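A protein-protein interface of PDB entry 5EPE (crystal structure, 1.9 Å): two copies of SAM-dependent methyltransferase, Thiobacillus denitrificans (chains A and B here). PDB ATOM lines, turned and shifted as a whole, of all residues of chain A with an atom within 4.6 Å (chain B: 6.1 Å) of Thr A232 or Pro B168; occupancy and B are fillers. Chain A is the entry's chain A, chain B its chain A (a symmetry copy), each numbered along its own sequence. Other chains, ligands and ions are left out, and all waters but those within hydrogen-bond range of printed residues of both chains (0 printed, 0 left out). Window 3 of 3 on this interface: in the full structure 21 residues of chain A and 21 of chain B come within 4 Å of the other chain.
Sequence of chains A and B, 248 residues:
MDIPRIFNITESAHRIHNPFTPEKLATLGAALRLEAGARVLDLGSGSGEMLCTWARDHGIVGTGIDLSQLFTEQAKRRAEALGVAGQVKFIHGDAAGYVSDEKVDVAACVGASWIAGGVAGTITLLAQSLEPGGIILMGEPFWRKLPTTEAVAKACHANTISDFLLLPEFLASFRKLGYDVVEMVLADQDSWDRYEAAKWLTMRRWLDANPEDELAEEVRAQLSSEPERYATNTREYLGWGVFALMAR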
ATOM      1  N   GLU A 228     -12.587 -13.439   1.757  1.00  0.00           N
ATOM      2  CA  GLU A 228     -13.786 -12.619   2.088  1.00  0.00           C
ATOM      3  C   GLU A 228     -15.028 -13.206   1.564  1.00  0.00           C
ATOM      4  O   GLU A 228     -16.021 -13.187   2.298  1.00  0.00           O
ATOM      5  CB  GLU A 228     -13.675 -11.182   1.554  1.00  0.00           C
ATOM      6  CG  GLU A 228     -12.725 -10.386   2.350  1.00  0.00           C
ATOM      7  CD  GLU A 228     -12.194  -9.227   1.523  1.00  0.00           C
ATOM      8  OE1 GLU A 228     -10.993  -9.278   1.237  1.00  0.00           O
ATOM      9  OE2 GLU A 228     -12.942  -8.250   1.196  1.00  0.00           O
ATOM     10  N   ARG A 229     -14.991 -13.733   0.341  1.00  0.00           N
ATOM     11  CA  ARG A 229     -16.139 -14.417  -0.234  1.00  0.00           C
ATOM     12  C   ARG A 229     -16.563 -15.598   0.661  1.00  0.00           C
ATOM     13  O   ARG A 229     -17.755 -15.774   0.961  1.00  0.00           O
ATOM     14  CB  ARG A 229     -15.849 -14.989  -1.649  1.00  0.00           C
ATOM     15  CG  ARG A 229     -17.098 -15.605  -2.347  1.00  0.00           C
ATOM     16  CD  ARG A 229     -16.974 -16.859  -3.274  1.00  0.00           C
ATOM     17  NE  ARG A 229     -16.209 -17.958  -2.688  1.00  0.00           N
ATOM     18  CZ  ARG A 229     -16.644 -18.841  -1.769  1.00  0.00           C
ATOM     19  NH1 ARG A 229     -15.791 -19.760  -1.277  1.00  0.00           N
ATOM     20  NH2 ARG A 229     -17.919 -18.825  -1.327  1.00  0.00           N
ATOM     21  N   TYR A 230     -15.589 -16.454   0.980  1.00  0.00           N
ATOM     22  CA  TYR A 230     -15.809 -17.617   1.841  1.00  0.00           C
ATOM     23  C   TYR A 230     -16.426 -17.197   3.201  1.00  0.00           C
ATOM     24  O   TYR A 230     -17.413 -17.765   3.640  1.00  0.00           O
ATOM     25  CB  TYR A 230     -14.474 -18.399   2.035  1.00  0.00           C
ATOM     26  CG  TYR A 230     -14.548 -19.351   3.156  1.00  0.00           C
ATOM     27  CD1 TYR A 230     -15.333 -20.490   3.050  1.00  0.00           C
ATOM     28  CD2 TYR A 230     -13.880 -19.104   4.354  1.00  0.00           C
ATOM     29  CE1 TYR A 230     -15.476 -21.347   4.109  1.00  0.00           C
ATOM     30  CE2 TYR A 230     -13.978 -19.979   5.413  1.00  0.00           C
ATOM     31  CZ  TYR A 230     -14.761 -21.127   5.289  1.00  0.00           C
ATOM     32  OH  TYR A 230     -14.933 -22.013   6.337  1.00  0.00           O
ATOM     33  N   ALA A 231     -15.834 -16.208   3.868  1.00  0.00           N
ATOM     34  CA  ALA A 231     -16.296 -15.794   5.189  1.00  0.00           C
ATOM     35  C   ALA A 231     -17.720 -15.176   5.148  1.00  0.00           C
ATOM     36  O   ALA A 231     -18.504 -15.389   6.040  1.00  0.00           O
ATOM     37  CB  ALA A 231     -15.318 -14.813   5.794  1.00  0.00           C
ATOM     38  N   THR A 232     -18.003 -14.394   4.125  1.00  0.00           N
ATOM     39  CA  THR A 232     -19.296 -13.740   3.967  1.00  0.00           C
ATOM     40  C   THR A 232     -20.415 -14.732   3.617  1.00  0.00           C
ATOM     41  O   THR A 232     -21.538 -14.617   4.119  1.00  0.00           O
ATOM     42  CB  THR A 232     -19.196 -12.630   2.875  1.00  0.00           C
ATOM     43  OG1 THR A 232     -18.200 -11.683   3.276  1.00  0.00           O
ATOM     44  CG2 THR A 232     -20.537 -11.898   2.592  1.00  0.00           C
ATOM     45  N   ASN A 233     -20.102 -15.689   2.747  1.00  0.00           N
ATOM     46  CA  ASN A 233     -21.112 -16.573   2.142  1.00  0.00           C
ATOM     47  C   ASN A 233     -21.021 -17.997   2.737  1.00  0.00           C
ATOM     48  O   ASN A 233     -21.778 -18.349   3.620  1.00  0.00           O
ATOM     49  CB  ASN A 233     -20.954 -16.525   0.616  1.00  0.00           C
ATOM     50  CG  ASN A 233     -21.148 -15.104   0.084  1.00  0.00           C
ATOM     51  OD1 ASN A 233     -22.221 -14.570   0.189  1.00  0.00           O
ATOM     52  ND2 ASN A 233     -20.111 -14.473  -0.346  1.00  0.00           N
ATOM     53  N   THR A 234     -20.032 -18.761   2.373  1.00  0.00           N
ATOM     54  CA  THR A 234     -20.009 -20.151   2.712  1.00  0.00           C
ATOM     55  C   THR A 234     -20.008 -20.374   4.213  1.00  0.00           C
ATOM     56  O   THR A 234     -20.763 -21.249   4.706  1.00  0.00           O
ATOM     57  CB  THR A 234     -18.777 -20.776   2.076  1.00  0.00           C
ATOM     58  OG1 THR A 234     -18.831 -20.468   0.676  1.00  0.00           O
ATOM     59  CG2 THR A 234     -18.665 -22.268   2.283  1.00  0.00           C
ATOM     60  N   TYR A 237     -23.457 -19.801   5.888  1.00  0.00           N
ATOM     61  CA  TYR A 237     -24.672 -20.296   5.250  1.00  0.00           C
ATOM     62  C   TYR A 237     -24.633 -21.733   4.735  1.00  0.00           C
ATOM     63  O   TYR A 237     -25.704 -22.365   4.666  1.00  0.00           O
ATOM     64  CB  TYR A 237     -25.013 -19.368   4.070  1.00  0.00           C
ATOM     65  CG  TYR A 237     -25.414 -18.033   4.533  1.00  0.00           C
ATOM     66  CD1 TYR A 237     -26.698 -17.802   5.046  1.00  0.00           C
ATOM     67  CD2 TYR A 237     -24.501 -16.958   4.480  1.00  0.00           C
ATOM     68  CE1 TYR A 237     -27.082 -16.547   5.502  1.00  0.00           C
ATOM     69  CE2 TYR A 237     -24.852 -15.703   4.952  1.00  0.00           C
ATOM     70  CZ  TYR A 237     -26.141 -15.502   5.433  1.00  0.00           C
ATOM     71  OH  TYR A 237     -26.495 -14.261   5.843  1.00  0.00           O
ATOM     72  N   LEU B 166     -16.108  -7.659  12.091  1.00  0.00           N
ATOM     73  CA  LEU B 166     -16.610  -8.968  11.728  1.00  0.00           C
ATOM     74  C   LEU B 166     -15.570  -9.655  10.826  1.00  0.00           C
ATOM     75  O   LEU B 166     -14.753  -8.982  10.178  1.00  0.00           O
ATOM     76  CB  LEU B 166     -17.975  -8.869  10.990  1.00  0.00           C
ATOM     77  CG  LEU B 166     -19.094  -8.386  11.920  1.00  0.00           C
ATOM     78  CD1 LEU B 166     -20.203  -7.845  11.026  1.00  0.00           C
ATOM     79  CD2 LEU B 166     -19.669  -9.520  12.742  1.00  0.00           C
ATOM     80  N   LEU B 167     -15.580 -10.988  10.807  1.00  0.00           N
ATOM     81  CA  LEU B 167     -14.541 -11.734  10.059  1.00  0.00           C
ATOM     82  C   LEU B 167     -14.296 -11.305   8.591  1.00  0.00           C
ATOM     83  O   LEU B 167     -13.150 -11.124   8.198  1.00  0.00           O
ATOM     84  CB  LEU B 167     -14.871 -13.235  10.103  1.00  0.00           C
ATOM     85  CG  LEU B 167     -13.795 -14.159   9.481  1.00  0.00           C
ATOM     86  CD1 LEU B 167     -12.436 -14.045  10.182  1.00  0.00           C
ATOM     87  CD2 LEU B 167     -14.243 -15.612   9.523  1.00  0.00           C
ATOM     88  N   PRO B 168     -15.361 -11.114   7.773  1.00  0.00           N
ATOM     89  CA  PRO B 168     -15.062 -10.678   6.406  1.00  0.00           C
ATOM     90  C   PRO B 168     -14.265  -9.352   6.363  1.00  0.00           C
ATOM     91  O   PRO B 168     -13.296  -9.237   5.629  1.00  0.00           O
ATOM     92  CB  PRO B 168     -16.450 -10.525   5.767  1.00  0.00           C
ATOM     93  CG  PRO B 168     -17.367 -11.351   6.584  1.00  0.00           C
ATOM     94  CD  PRO B 168     -16.813 -11.289   7.994  1.00  0.00           C
ATOM     95  N   GLU B 169     -14.673  -8.373   7.175  1.00  0.00           N
ATOM     96  CA  GLU B 169     -14.009  -7.069   7.195  1.00  0.00           C
ATOM     97  C   GLU B 169     -12.609  -7.196   7.816  1.00  0.00           C
ATOM     98  O   GLU B 169     -11.667  -6.490   7.396  1.00  0.00           O
ATOM     99  CB  GLU B 169     -14.838  -6.062   7.995  1.00  0.00           C
ATOM    100  CG  GLU B 169     -16.072  -5.444   7.283  1.00  0.00           C
ATOM    101  CD  GLU B 169     -17.278  -6.434   7.055  1.00  0.00           C
ATOM    102  OE1 GLU B 169     -17.443  -7.490   7.756  1.00  0.00           O
ATOM    103  OE2 GLU B 169     -18.133  -6.081   6.194  1.00  0.00           O
ATOM    104  N   PHE B 170     -12.465  -8.095   8.768  1.00  0.00           N
ATOM    105  CA  PHE B 170     -11.153  -8.331   9.381  1.00  0.00           C
ATOM    106  C   PHE B 170     -10.184  -8.947   8.370  1.00  0.00           C
ATOM    107  O   PHE B 170      -9.052  -8.481   8.204  1.00  0.00           O
ATOM    108  CB  PHE B 170     -11.263  -9.206  10.655  1.00  0.00           C
ATOM    109  CG  PHE B 170      -9.985  -9.199  11.477  1.00  0.00           C
ATOM    110  CD1 PHE B 170      -9.370  -8.005  11.811  1.00  0.00           C
ATOM    111  CD2 PHE B 170      -9.400 -10.387  11.895  1.00  0.00           C
ATOM    112  CE1 PHE B 170      -8.209  -7.956  12.549  1.00  0.00           C
ATOM    113  CE2 PHE B 170      -8.250 -10.341  12.663  1.00  0.00           C
ATOM    114  CZ  PHE B 170      -7.636  -9.138  12.963  1.00  0.00           C
ATOM    115  N   LEU B 171     -10.634  -9.978   7.669  1.00  0.00           N
ATOM    116  CA  LEU B 171      -9.858 -10.519   6.554  1.00  0.00           C
ATOM    117  C   LEU B 171      -9.524  -9.478   5.506  1.00  0.00           C
ATOM    118  O   LEU B 171      -8.371  -9.403   5.049  1.00  0.00           O
ATOM    119  CB  LEU B 171     -10.562 -11.718   5.929  1.00  0.00           C
ATOM    120  CG  LEU B 171     -10.659 -12.955   6.824  1.00  0.00           C
ATOM    121  CD1 LEU B 171     -11.676 -13.910   6.231  1.00  0.00           C
ATOM    122  CD2 LEU B 171      -9.281 -13.576   6.932  1.00  0.00           C
ATOM    123  N   ALA B 172     -10.513  -8.662   5.140  1.00  0.00           N
ATOM    124  CA  ALA B 172     -10.275  -7.516   4.249  1.00  0.00           C
ATOM    125  C   ALA B 172      -9.204  -6.587   4.778  1.00  0.00           C
ATOM    126  O   ALA B 172      -8.439  -6.032   3.977  1.00  0.00           O
ATOM    127  CB  ALA B 172     -11.546  -6.744   3.976  1.00  0.00           C
ATOM    128  N   SER B 173      -9.151  -6.364   6.099  1.00  0.00           N
ATOM    129  CA  SER B 173      -8.153  -5.451   6.625  1.00  0.00           C
ATOM    130  C   SER B 173      -6.709  -5.939   6.355  1.00  0.00           C
ATOM    131  O   SER B 173      -5.820  -5.099   6.049  1.00  0.00           O
ATOM    132  CB  SER B 173      -8.327  -5.182   8.127  1.00  0.00           C
ATOM    133  OG  SER B 173      -8.052  -6.293   8.952  1.00  0.00           O
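The backbone carbonyl oxygen (O) of Glu A228 sits at hydrogen-bond distance from the side-chain hydroxyl (OG1) of Thr A232, 2.8 Å away.
Among the printed residues, merely in contact across the chains: Glu A228 with Pro B168 (3.5 Å), Glu A228 with Ala B172 (3.5 Å), Ala A231 with Leu B167 (3.96 Å), Ala A231 with Leu B171 (3.8 Å) and Thr A232 with Pro B168 (3.3 Å).
Of chain B, only Pro B168 comes within 4 Å of Thr A232. Pro B168 touches just these residues of chain A: Glu A228 and Thr A232. Of the printed residues of chain B, Glu A228 touches Pro B168 (3.5 Å) and Ala B172 (3.5 Å). Of the printed residues of chain B, Ala A231 touches Leu B167 (3.96 Å) and Leu B171 (3.8 Å). The nearest printed residue of chain B that does not touch Thr A232 is Glu B169 (6.2 Å).
Of the 8 printed residues of chain A, 3 touch a printed residue of chain B. Hydrophobic or aromatic side chains of chain A within 4 Å of the printed part of chain B: Ala A231.
No position is printed for both chains.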
